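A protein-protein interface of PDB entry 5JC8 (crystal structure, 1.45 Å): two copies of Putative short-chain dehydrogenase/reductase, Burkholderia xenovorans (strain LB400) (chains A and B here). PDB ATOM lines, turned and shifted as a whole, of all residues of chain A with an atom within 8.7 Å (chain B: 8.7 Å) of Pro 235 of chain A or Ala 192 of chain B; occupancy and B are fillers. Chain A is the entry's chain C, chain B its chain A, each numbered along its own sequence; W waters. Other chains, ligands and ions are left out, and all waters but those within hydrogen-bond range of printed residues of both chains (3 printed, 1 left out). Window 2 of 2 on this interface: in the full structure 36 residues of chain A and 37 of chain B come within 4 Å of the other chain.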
ATOM      1  N   ARG A 230       1.796  36.054   7.985  1.00  0.00           N
ATOM      2  CA  ARG A 230       0.976  35.280   8.911  1.00  0.00           C
ATOM      3  C   ARG A 230       1.629  33.935   9.202  1.00  0.00           C
ATOM      4  O   ARG A 230       1.673  33.493  10.355  1.00  0.00           O
ATOM      5  CB  ARG A 230      -0.438  35.101   8.347  1.00  0.00           C
ATOM      6  CG  ARG A 230      -1.272  36.396   8.332  1.00  0.00           C
ATOM      7  CD  ARG A 230      -2.469  36.325   7.369  1.00  0.00           C
ATOM      8  NE  ARG A 230      -3.445  35.279   7.676  1.00  0.00           N
ATOM      9  CZ  ARG A 230      -4.486  35.430   8.490  1.00  0.00           C
ATOM     10  NH1 ARG A 230      -4.710  36.595   9.085  1.00  0.00           N
ATOM     11  NH2 ARG A 230      -5.320  34.417   8.696  1.00  0.00           N
ATOM     12  N   GLN A 231       2.174  33.292   8.164  1.00  0.00           N
ATOM     13  CA  GLN A 231       2.820  31.995   8.337  1.00  0.00           C
ATOM     14  C   GLN A 231       4.001  32.072   9.295  1.00  0.00           C
ATOM     15  O   GLN A 231       4.281  31.102  10.004  1.00  0.00           O
ATOM     16  CB  GLN A 231       3.302  31.470   6.983  1.00  0.00           C
ATOM     17  CG  GLN A 231       3.827  30.029   7.053  1.00  0.00           C
ATOM     18  CD  GLN A 231       2.759  29.029   7.466  1.00  0.00           C
ATOM     19  OE1 GLN A 231       1.676  28.987   6.879  1.00  0.00           O
ATOM     20  NE2 GLN A 231       3.048  28.242   8.499  1.00  0.00           N
ATOM     21  N   ALA A 232       4.712  33.204   9.324  1.00  0.00           N
ATOM     22  CA  ALA A 232       5.862  33.335  10.213  1.00  0.00           C
ATOM     23  C   ALA A 232       5.469  33.259  11.682  1.00  0.00           C
ATOM     24  O   ALA A 232       6.334  33.029  12.533  1.00  0.00           O
ATOM     25  CB  ALA A 232       6.545  34.674   9.957  1.00  0.00           C
ATOM     26  N   ARG A 233       4.192  33.454  12.000  1.00  0.00           N
ATOM     27  CA  ARG A 233       3.698  33.360  13.360  1.00  0.00           C
ATOM     28  C   ARG A 233       3.302  31.946  13.741  1.00  0.00           C
ATOM     29  O   ARG A 233       2.993  31.683  14.915  1.00  0.00           O
ATOM     30  CB  ARG A 233       2.471  34.258  13.489  1.00  0.00           C
ATOM     31  CG  ARG A 233       2.780  35.689  13.177  1.00  0.00           C
ATOM     32  CD  ARG A 233       1.535  36.510  13.055  1.00  0.00           C
ATOM     33  NE  ARG A 233       1.893  37.855  12.665  1.00  0.00           N
ATOM     34  CZ  ARG A 233       1.083  38.690  12.032  1.00  0.00           C
ATOM     35  NH1 ARG A 233      -0.152  38.311  11.732  1.00  0.00           N
ATOM     36  NH2 ARG A 233       1.514  39.901  11.709  1.00  0.00           N
ATOM     37  N   ILE A 234       3.262  31.041  12.774  1.00  0.00           N
ATOM     38  CA  ILE A 234       2.697  29.709  12.946  1.00  0.00           C
ATOM     39  C   ILE A 234       3.845  28.708  13.007  1.00  0.00           C
ATOM     40  O   ILE A 234       4.580  28.557  12.022  1.00  0.00           O
ATOM     41  CB  ILE A 234       1.738  29.381  11.790  1.00  0.00           C
ATOM     42  CG1 ILE A 234       0.547  30.349  11.799  1.00  0.00           C
ATOM     43  CG2 ILE A 234       1.256  27.942  11.888  1.00  0.00           C
ATOM     44  CD1 ILE A 234      -0.285  30.286  10.528  1.00  0.00           C
ATOM     45  N   PRO A 235       4.038  28.005  14.125  1.00  0.00           N
ATOM     46  CA  PRO A 235       5.121  27.003  14.166  1.00  0.00           C
ATOM     47  C   PRO A 235       4.954  25.868  13.164  1.00  0.00           C
ATOM     48  O   PRO A 235       5.943  25.443  12.549  1.00  0.00           O
ATOM     49  CB  PRO A 235       5.086  26.530  15.626  1.00  0.00           C
ATOM     50  CG  PRO A 235       4.582  27.732  16.361  1.00  0.00           C
ATOM     51  CD  PRO A 235       3.544  28.340  15.473  1.00  0.00           C
ATOM     52  N   MET A 236       3.741  25.355  12.990  1.00  0.00           N
ATOM     53  CA  MET A 236       3.521  24.297  12.012  1.00  0.00           C
ATOM     54  C   MET A 236       3.821  24.823  10.610  1.00  0.00           C
ATOM     55  O   MET A 236       3.536  25.986  10.313  1.00  0.00           O
ATOM     56  CB  MET A 236       2.073  23.795  12.070  1.00  0.00           C
ATOM     57  CG  MET A 236       1.690  22.963  13.309  1.00  0.00           C
ATOM     58  SD  MET A 236       2.668  21.461  13.582  1.00  0.00           S
ATOM     59  CE  MET A 236       2.098  20.411  12.238  1.00  0.00           C
ATOM     60  N   PRO A 237       4.376  23.990   9.734  1.00  0.00           N
ATOM     61  CA  PRO A 237       4.832  24.465   8.416  1.00  0.00           C
ATOM     62  C   PRO A 237       3.762  24.618   7.339  1.00  0.00           C
ATOM     63  O   PRO A 237       4.069  24.481   6.147  1.00  0.00           O
ATOM     64  CB  PRO A 237       5.917  23.447   8.025  1.00  0.00           C
ATOM     65  CG  PRO A 237       5.547  22.199   8.757  1.00  0.00           C
ATOM     66  CD  PRO A 237       4.833  22.619  10.027  1.00  0.00           C
ATOM     67  N   PHE A 238       2.509  24.827   7.731  1.00  0.00           N
ATOM     68  CA  PHE A 238       1.437  25.102   6.780  1.00  0.00           C
ATOM     69  C   PHE A 238       0.412  25.989   7.471  1.00  0.00           C
ATOM     70  O   PHE A 238       0.531  26.292   8.663  1.00  0.00           O
ATOM     71  CB  PHE A 238       0.797  23.804   6.257  1.00  0.00           C
ATOM     72  CG  PHE A 238      -0.098  23.119   7.244  1.00  0.00           C
ATOM     73  CD1 PHE A 238       0.430  22.399   8.311  1.00  0.00           C
ATOM     74  CD2 PHE A 238      -1.470  23.186   7.106  1.00  0.00           C
ATOM     75  CE1 PHE A 238      -0.400  21.760   9.206  1.00  0.00           C
ATOM     76  CE2 PHE A 238      -2.313  22.542   7.991  1.00  0.00           C
ATOM     77  CZ  PHE A 238      -1.775  21.836   9.058  1.00  0.00           C
ATOM     78  N   MET A 239      -0.592  26.439   6.712  1.00  0.00           N
ATOM     79  CA  MET A 239      -1.700  27.200   7.276  1.00  0.00           C
ATOM     80  C   MET A 239      -2.984  26.405   7.079  1.00  0.00           C
ATOM     81  O   MET A 239      -3.260  25.940   5.968  1.00  0.00           O
ATOM     82  CB  MET A 239      -1.808  28.581   6.615  1.00  0.00           C
ATOM     83  CG  MET A 239      -2.886  29.471   7.219  1.00  0.00           C
ATOM     84  SD  MET A 239      -2.930  31.093   6.435  1.00  0.00           S
ATOM     85  CE  MET A 239      -1.343  31.741   6.983  1.00  0.00           C
ATOM     86  N   ASP A 268      -4.585  26.447  15.860  1.00  0.00           N
ATOM     87  CA  ASP A 268      -3.775  27.585  15.447  1.00  0.00           C
ATOM     88  C   ASP A 268      -2.352  27.209  15.055  1.00  0.00           C
ATOM     89  O   ASP A 268      -1.505  28.109  14.967  1.00  0.00           O
ATOM     90  CB  ASP A 268      -3.772  28.661  16.547  1.00  0.00           C
ATOM     91  CG  ASP A 268      -2.916  28.285  17.760  1.00  0.00           C
ATOM     92  OD1 ASP A 268      -2.436  27.140  17.906  1.00  0.00           O
ATOM     93  OD2 ASP A 268      -2.741  29.191  18.595  1.00  0.00           O
ATOM     94  N   GLY A 269      -2.042  25.931  14.839  1.00  0.00           N
ATOM     95  CA  GLY A 269      -0.708  25.561  14.422  1.00  0.00           C
ATOM     96  C   GLY A 269       0.381  25.803  15.443  1.00  0.00           C
ATOM     97  O   GLY A 269       1.560  25.793  15.074  1.00  0.00           O
ATOM     98  N   GLY A 270       0.019  26.033  16.713  1.00  0.00           N
ATOM     99  CA  GLY A 270       0.978  26.299  17.772  1.00  0.00           C
ATOM    100  C   GLY A 270       1.232  27.763  18.062  1.00  0.00           C
ATOM    101  O   GLY A 270       2.022  28.071  18.964  1.00  0.00           O
ATOM    102  N   MET A 271       0.557  28.671  17.349  1.00  0.00           N
ATOM    103  CA  MET A 271       0.883  30.093  17.420  1.00  0.00           C
ATOM    104  C   MET A 271       0.759  30.654  18.833  1.00  0.00           C
ATOM    105  O   MET A 271       1.641  31.392  19.294  1.00  0.00           O
ATOM    106  CB  MET A 271      -0.035  30.846  16.469  1.00  0.00           C
ATOM    107  CG  MET A 271       0.137  32.352  16.517  1.00  0.00           C
ATOM    108  SD  MET A 271      -1.061  33.230  15.475  1.00  0.00           S
ATOM    109  CE  MET A 271      -2.617  32.946  16.330  1.00  0.00           C
ATOM    110  N   SER A 272      -0.328  30.347  19.531  1.00  0.00           N
ATOM    111  CA  SER A 272      -0.519  31.009  20.814  1.00  0.00           C
ATOM    112  C   SER A 272       0.388  30.463  21.906  1.00  0.00           C
ATOM    113  O   SER A 272       0.495  31.103  22.960  1.00  0.00           O
ATOM    114  CB  SER A 272      -1.976  30.959  21.245  1.00  0.00           C
ATOM    115  OG  SER A 272      -2.413  29.628  21.279  1.00  0.00           O
ATOM    116  N   ALA A 273       1.075  29.350  21.666  1.00  0.00           N
ATOM    117  CA  ALA A 273       2.025  28.790  22.626  1.00  0.00           C
ATOM    118  C   ALA A 273       3.374  29.496  22.613  1.00  0.00           C
ATOM    119  O   ALA A 273       4.209  29.225  23.483  1.00  0.00           O
ATOM    120  CB  ALA A 273       2.227  27.297  22.367  1.00  0.00           C
ATOM    121  N   ARG A 274       3.621  30.374  21.645  1.00  0.00           N
ATOM    122  CA  ARG A 274       4.903  31.044  21.497  1.00  0.00           C
ATOM    123  C   ARG A 274       4.732  32.552  21.548  1.00  0.00           C
ATOM    124  O   ARG A 274       3.676  33.091  21.199  1.00  0.00           O
ATOM    125  CB  ARG A 274       5.623  30.643  20.185  1.00  0.00           C
ATOM    126  CG  ARG A 274       4.747  30.682  18.911  1.00  0.00           C
ATOM    127  CD  ARG A 274       5.556  31.075  17.644  1.00  0.00           C
ATOM    128  NE  ARG A 274       5.978  32.467  17.796  1.00  0.00           N
ATOM    129  CZ  ARG A 274       5.210  33.516  17.515  1.00  0.00           C
ATOM    130  NH1 ARG A 274       4.006  33.352  16.973  1.00  0.00           N
ATOM    131  NH2 ARG A 274       5.653  34.729  17.785  1.00  0.00           N
ATOM    132  N   CYS A 275       5.789  33.216  21.993  1.00  0.00           N
ATOM    133  CA  CYS A 275       5.872  34.672  21.987  1.00  0.00           C
ATOM    134  C   CYS A 275       7.273  35.125  21.604  1.00  0.00           C
ATOM    135  O   CYS A 275       7.707  36.230  21.969  1.00  0.00           O
ATOM    136  CB  CYS A 275       5.405  35.254  23.326  1.00  0.00           C
ATOM    137  SG  CYS A 275       6.371  34.685  24.757  1.00  0.00           S
ATOM    138  N   ASP A 276       7.994  34.284  20.866  1.00  0.00           N
ATOM    139  CA  ASP A 276       9.311  34.681  20.386  1.00  0.00           C
ATOM    140  C   ASP A 276       9.218  35.532  19.128  1.00  0.00           C
ATOM    141  O   ASP A 276      10.236  35.817  18.519  1.00  0.00           O
ATOM    142  CB  ASP A 276      10.243  33.476  20.176  1.00  0.00           C
ATOM    143  CG  ASP A 276       9.751  32.511  19.122  1.00  0.00           C
ATOM    144  OD1 ASP A 276       8.547  32.508  18.801  1.00  0.00           O
ATOM    145  OD2 ASP A 276      10.590  31.720  18.642  1.00  0.00           O
ATOM    146  OXT ASP A 276       8.117  35.923  18.717  1.00  0.00           O
ATOM    147  N   GLU B 146      11.106  12.754  13.742  1.00  0.00           N
ATOM    148  CA  GLU B 146      11.771  13.727  12.881  1.00  0.00           C
ATOM    149  C   GLU B 146      12.273  13.073  11.601  1.00  0.00           C
ATOM    150  O   GLU B 146      12.070  13.595  10.496  1.00  0.00           O
ATOM    151  CB  GLU B 146      12.926  14.392  13.628  1.00  0.00           C
ATOM    152  CG  GLU B 146      13.682  15.398  12.775  1.00  0.00           C
ATOM    153  CD  GLU B 146      14.693  16.213  13.556  1.00  0.00           C
ATOM    154  OE1 GLU B 146      15.624  16.747  12.915  1.00  0.00           O
ATOM    155  OE2 GLU B 146      14.562  16.321  14.793  1.00  0.00           O
ATOM    156  N   GLY B 149       9.517  12.057   9.017  1.00  0.00           N
ATOM    157  CA  GLY B 149       8.718  13.111   8.430  1.00  0.00           C
ATOM    158  C   GLY B 149       7.565  13.626   9.260  1.00  0.00           C
ATOM    159  O   GLY B 149       6.783  14.440   8.753  1.00  0.00           O
ATOM    160  N   GLY B 150       7.432  13.192  10.503  1.00  0.00           N
ATOM    161  CA  GLY B 150       6.429  13.751  11.386  1.00  0.00           C
ATOM    162  C   GLY B 150       5.881  12.717  12.347  1.00  0.00           C
ATOM    163  O   GLY B 150       6.273  11.548  12.345  1.00  0.00           O
ATOM    164  N   ARG B 184       3.795  21.840  25.466  1.00  0.00           N
ATOM    165  CA  ARG B 184       3.723  23.073  24.691  1.00  0.00           C
ATOM    166  C   ARG B 184       5.072  23.439  24.095  1.00  0.00           C
ATOM    167  O   ARG B 184       5.146  23.854  22.928  1.00  0.00           O
ATOM    168  CB  ARG B 184       3.222  24.220  25.559  1.00  0.00           C
ATOM    169  CG  ARG B 184       1.797  24.042  26.049  1.00  0.00           C
ATOM    170  CD  ARG B 184       1.312  25.310  26.679  1.00  0.00           C
ATOM    171  NE  ARG B 184       0.014  25.167  27.341  1.00  0.00           N
ATOM    172  CZ  ARG B 184      -0.177  25.329  28.647  1.00  0.00           C
ATOM    173  NH1 ARG B 184       0.849  25.641  29.436  1.00  0.00           N
ATOM    174  NH2 ARG B 184      -1.395  25.200  29.166  1.00  0.00           N
ATOM    175  N   VAL B 185       6.149  23.339  24.885  1.00  0.00           N
ATOM    176  CA  VAL B 185       7.448  23.793  24.403  1.00  0.00           C
ATOM    177  C   VAL B 185       8.057  22.798  23.420  1.00  0.00           C
ATOM    178  O   VAL B 185       8.765  23.195  22.485  1.00  0.00           O
ATOM    179  CB  VAL B 185       8.412  24.217  25.531  1.00  0.00           C
ATOM    180  CG1 VAL B 185       7.816  25.379  26.336  1.00  0.00           C
ATOM    181  CG2 VAL B 185       8.802  23.048  26.454  1.00  0.00           C
ATOM    182  N   VAL B 186       7.785  21.504  23.602  1.00  0.00           N
ATOM    183  CA  VAL B 186       8.198  20.530  22.597  1.00  0.00           C
ATOM    184  C   VAL B 186       7.413  20.746  21.310  1.00  0.00           C
ATOM    185  O   VAL B 186       7.970  20.660  20.202  1.00  0.00           O
ATOM    186  CB  VAL B 186       8.059  19.097  23.148  1.00  0.00           C
ATOM    187  CG1 VAL B 186       8.370  18.054  22.068  1.00  0.00           C
ATOM    188  CG2 VAL B 186       8.992  18.920  24.338  1.00  0.00           C
ATOM    189  N   ALA B 187       6.115  21.072  21.435  1.00  0.00           N
ATOM    190  CA  ALA B 187       5.329  21.376  20.243  1.00  0.00           C
ATOM    191  C   ALA B 187       5.951  22.517  19.447  1.00  0.00           C
ATOM    192  O   ALA B 187       6.102  22.423  18.225  1.00  0.00           O
ATOM    193  CB  ALA B 187       3.895  21.728  20.638  1.00  0.00           C
ATOM    194  N   VAL B 188       6.323  23.615  20.117  1.00  0.00           N
ATOM    195  CA  VAL B 188       6.887  24.735  19.374  1.00  0.00           C
ATOM    196  C   VAL B 188       8.226  24.348  18.756  1.00  0.00           C
ATOM    197  O   VAL B 188       8.487  24.636  17.583  1.00  0.00           O
ATOM    198  CB  VAL B 188       6.993  25.996  20.252  1.00  0.00           C
ATOM    199  CG1 VAL B 188       7.671  27.114  19.470  1.00  0.00           C
ATOM    200  CG2 VAL B 188       5.603  26.430  20.715  1.00  0.00           C
ATOM    201  N   GLU B 189       9.066  23.635  19.513  1.00  0.00           N
ATOM    202  CA  GLU B 189      10.404  23.315  19.031  1.00  0.00           C
ATOM    203  C   GLU B 189      10.373  22.380  17.823  1.00  0.00           C
ATOM    204  O   GLU B 189      11.195  22.516  16.911  1.00  0.00           O
ATOM    205  CB  GLU B 189      11.259  22.718  20.160  1.00  0.00           C
ATOM    206  CG  GLU B 189      12.689  22.477  19.680  1.00  0.00           C
ATOM    207  CD  GLU B 189      13.643  21.952  20.718  1.00  0.00           C
ATOM    208  OE1 GLU B 189      13.193  21.511  21.792  1.00  0.00           O
ATOM    209  OE2 GLU B 189      14.869  21.984  20.427  1.00  0.00           O
ATOM    210  N   TYR B 190       9.424  21.437  17.794  1.00  0.00           N
ATOM    211  CA  TYR B 190       9.415  20.384  16.780  1.00  0.00           C
ATOM    212  C   TYR B 190       8.343  20.572  15.720  1.00  0.00           C
ATOM    213  O   TYR B 190       8.240  19.739  14.816  1.00  0.00           O
ATOM    214  CB  TYR B 190       9.306  18.995  17.443  1.00  0.00           C
ATOM    215  CG  TYR B 190      10.633  18.579  18.023  1.00  0.00           C
ATOM    216  CD1 TYR B 190      11.037  19.029  19.279  1.00  0.00           C
ATOM    217  CD2 TYR B 190      11.508  17.763  17.299  1.00  0.00           C
ATOM    218  CE1 TYR B 190      12.275  18.682  19.796  1.00  0.00           C
ATOM    219  CE2 TYR B 190      12.745  17.416  17.811  1.00  0.00           C
ATOM    220  CZ  TYR B 190      13.122  17.879  19.057  1.00  0.00           C
ATOM    221  OH  TYR B 190      14.356  17.531  19.563  1.00  0.00           O
ATOM    222  N   ALA B 191       7.574  21.661  15.780  1.00  0.00           N
ATOM    223  CA  ALA B 191       6.546  21.904  14.772  1.00  0.00           C
ATOM    224  C   ALA B 191       7.126  21.930  13.364  1.00  0.00           C
ATOM    225  O   ALA B 191       6.506  21.414  12.432  1.00  0.00           O
ATOM    226  CB  ALA B 191       5.851  23.229  15.068  1.00  0.00           C
ATOM    227  N   ALA B 192       8.307  22.521  13.182  1.00  0.00           N
ATOM    228  CA  ALA B 192       8.874  22.585  11.840  1.00  0.00           C
ATOM    229  C   ALA B 192       9.205  21.209  11.286  1.00  0.00           C
ATOM    230  O   ALA B 192       9.371  21.073  10.067  1.00  0.00           O
ATOM    231  CB  ALA B 192      10.133  23.452  11.814  1.00  0.00           C
ATOM    232  N   LYS B 193       9.345  20.201  12.150  1.00  0.00           N
ATOM    233  CA  LYS B 193       9.582  18.824  11.736  1.00  0.00           C
ATOM    234  C   LYS B 193       8.286  18.033  11.604  1.00  0.00           C
ATOM    235  O   LYS B 193       8.331  16.798  11.509  1.00  0.00           O
ATOM    236  CB  LYS B 193      10.540  18.133  12.714  1.00  0.00           C
ATOM    237  CG  LYS B 193      11.864  18.876  12.881  1.00  0.00           C
ATOM    238  CD  LYS B 193      12.617  18.935  11.566  1.00  0.00           C
ATOM    239  CE  LYS B 193      13.988  19.580  11.722  1.00  0.00           C
ATOM    240  NZ  LYS B 193      14.479  19.509  13.124  1.00  0.00           N
ATOM    241  N   ASN B 194       7.139  18.719  11.621  1.00  0.00           N
ATOM    242  CA  ASN B 194       5.823  18.100  11.452  1.00  0.00           C
ATOM    243  C   ASN B 194       5.484  17.154  12.599  1.00  0.00           C
ATOM    244  O   ASN B 194       4.784  16.151  12.413  1.00  0.00           O
ATOM    245  CB  ASN B 194       5.688  17.409  10.085  1.00  0.00           C
ATOM    246  CG  ASN B 194       4.236  17.128   9.699  1.00  0.00           C
ATOM    247  OD1 ASN B 194       3.328  17.902  10.009  1.00  0.00           O
ATOM    248  ND2 ASN B 194       4.019  16.007   9.007  1.00  0.00           N
ATOM    249  N   VAL B 195       5.978  17.459  13.792  1.00  0.00           N
ATOM    250  CA  VAL B 195       5.620  16.721  14.996  1.00  0.00           C
ATOM    251  C   VAL B 195       4.681  17.599  15.798  1.00  0.00           C
ATOM    252  O   VAL B 195       5.038  18.727  16.145  1.00  0.00           O
ATOM    253  CB  VAL B 195       6.861  16.369  15.828  1.00  0.00           C
ATOM    254  CG1 VAL B 195       6.444  15.609  17.087  1.00  0.00           C
ATOM    255  CG2 VAL B 195       7.841  15.560  15.023  1.00  0.00           C
ATOM    256  N   ARG B 196       3.491  17.092  16.100  1.00  0.00           N
ATOM    257  CA  ARG B 196       2.534  17.803  16.936  1.00  0.00           C
ATOM    258  C   ARG B 196       2.557  17.229  18.344  1.00  0.00           C
ATOM    259  O   ARG B 196       2.785  16.028  18.524  1.00  0.00           O
ATOM    260  CB  ARG B 196       1.108  17.676  16.389  1.00  0.00           C
ATOM    261  CG  ARG B 196       0.966  18.284  14.991  1.00  0.00           C
ATOM    262  CD  ARG B 196      -0.489  18.273  14.486  1.00  0.00           C
ATOM    263  NE  ARG B 196      -0.975  16.906  14.358  1.00  0.00           N
ATOM    264  CZ  ARG B 196      -1.765  16.299  15.242  1.00  0.00           C
ATOM    265  NH1 ARG B 196      -2.184  16.947  16.320  1.00  0.00           N
ATOM    266  NH2 ARG B 196      -2.127  15.042  15.050  1.00  0.00           N
ATOM    267  N   PHE B 259      -3.647  20.716  12.379  1.00  0.00           N
ATOM    268  CA  PHE B 259      -3.282  22.095  12.695  1.00  0.00           C
ATOM    269  C   PHE B 259      -3.424  22.392  14.183  1.00  0.00           C
ATOM    270  O   PHE B 259      -3.437  23.561  14.585  1.00  0.00           O
ATOM    271  CB  PHE B 259      -4.131  23.051  11.840  1.00  0.00           C
ATOM    272  CG  PHE B 259      -3.570  24.447  11.711  1.00  0.00           C
ATOM    273  CD1 PHE B 259      -2.281  24.659  11.226  1.00  0.00           C
ATOM    274  CD2 PHE B 259      -4.359  25.558  12.025  1.00  0.00           C
ATOM    275  CE1 PHE B 259      -1.779  25.963  11.069  1.00  0.00           C
ATOM    276  CE2 PHE B 259      -3.856  26.865  11.876  1.00  0.00           C
ATOM    277  CZ  PHE B 259      -2.572  27.052  11.406  1.00  0.00           C
ATOM    278  N   THR B 261      -1.710  22.011  17.740  1.00  0.00           N
ATOM    279  CA  THR B 261      -0.495  21.636  18.445  1.00  0.00           C
ATOM    280  C   THR B 261      -0.225  22.653  19.544  1.00  0.00           C
ATOM    281  O   THR B 261      -0.630  23.823  19.453  1.00  0.00           O
ATOM    282  CB  THR B 261       0.706  21.473  17.496  1.00  0.00           C
ATOM    283  OG1 THR B 261       1.757  20.787  18.175  1.00  0.00           O
ATOM    284  CG2 THR B 261       1.238  22.811  16.998  1.00  0.00           C
ATOM    285  N   GLY B 262       0.472  22.189  20.580  1.00  0.00           N
ATOM    286  CA  GLY B 262       0.809  23.073  21.681  1.00  0.00           C
ATOM    287  C   GLY B 262      -0.339  23.420  22.594  1.00  0.00           C
ATOM    288  O   GLY B 262      -0.281  24.446  23.273  1.00  0.00           O
HETATM  289  O   HOH W   1      -3.505  24.525  17.949  1.00  0.00           O
HETATM  290  O   HOH W   2      -1.520  27.137  22.967  1.00  0.00           O
HETATM  291  O   HOH W   3      -1.405  26.423  20.411  1.00  0.00           O
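Printed residues of chain A that touch a printed residue of chain B: Ile 234, Pro 235, Met 236, Pro 237, Phe 238, Met 239, Asp 268, Gly 269, Gly 270 and Ala 273. Hydrophobic or aromatic side chains of chain A that line the printed part of chain B: Ile 234, Pro 235, Met 236, Pro 237, Phe 238 and Ala 273. Hydrophobic or aromatic side chains of chain B that line the printed part of chain A: Val 188, Ala 191 and Phe 259.
NE2 of Gln 231 of chain A lies within hydrogen-bond range of O of Phe 238 of chain A, at 3.2 Å. The side-chain carboxylate of Asp 268 of chain A is in hydrogen-bond range of the side-chain hydroxyl of Ser 272 of chain A (2.7 Å). The backbone NH (N) of Gly 270 of chain A sits at hydrogen-bond distance from the side-chain carboxylate (OD1) of Asp 268 of chain A, 2.9 Å away. OE1 of Gln 231 of chain A is in hydrogen-bond range of N of Met 239 of chain A, at 3.4 Å. The backbone carbonyl oxygen (O) of Gly 149 of chain B is in hydrogen-bond range of the side-chain amide nitrogen (ND2) of Asn 194 of chain B (3.2 Å). The backbone carbonyl oxygen (O) of Met 236 of chain A sits at hydrogen-bond distance from the side-chain amide nitrogen (NE2) of Gln 231 of chain A.
Water W3 lies within hydrogen-bond range of OD1 of Asp 268 of chain A (2.8 Å), O of Thr 261 of chain B (2.9 Å) and OG of Ser 272 of chain A (3.5 Å). Water W2 lies within hydrogen-bond range of O of Gly 262 of chain B (3.0 Å) and OG of Ser 272 of chain A (3.1 Å).
Among the printed residues, pairs that only touch across the chains: Pro 237 of chain A with Ala 191 of chain B, Phe 238 of chain A with Phe 259 of chain B, Pro 235 of chain A with Ala 191 of chain B, Gly 270 of chain A with Thr 261 of chain B, Gly 269 of chain A with Thr 261 of chain B, Met 236 of chain A with Asn 194 of chain B, Met 236 of chain A with Ala 191 of chain B, Met 236 of chain A with Arg 196 of chain B, Ile 234 of chain A with Phe 259 of chain B, Met 236 of chain A with Thr 261 of chain B, Pro 235 of chain A with Ala 192 of chain B, Ala 273 of chain A with Val 188 of chain B, Ala 273 of chain A with Gly 262 of chain B and Met 239 of chain A with Phe 259 of chain B.
No position is printed for both chains. Of the 16 pairs that touch across the chains among the printed residues, none has its exchanged pair printed and touching as well.
O of Phe 259 of chain B sits at hydrogen-bond distance from N of Gly 269 of chain A (2.8 Å). The backbone carbonyl oxygen of Phe 259 of chain B lies within hydrogen-bond range of the backbone NH of Asp 268 of chain A (3.4 Å).
Of chain B, only Ala 191 (3.4 Å) and Ala 192 (3.8 Å) come within 4 Å of Pro 235 of chain A. Printed residues of chain B within 4 Å of Pro 237 of chain A: Ala 191. Of the printed residues of chain B, Phe 238 of chain A touches Phe 259. Of the printed residues of chain B, Met 239 of chain A touches Phe 259 (3.99 Å). Gly 270 of chain A touches just one residue of chain B: Thr 261 (3.4 Å). Met 271 of chain A touches none of the printed residues of chain B. Glu 189 of chain B touches none of the printed residues of chain A. Ala 192 of chain B touches just one residue of chain A: Pro 235 (3.8 Å). Of the printed residues of chain A, Gly 262 of chain B touches Ala 273. The nearest residue of chain B that does not touch Pro 235 of chain A is Val 188 of chain B (4.4 Å).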
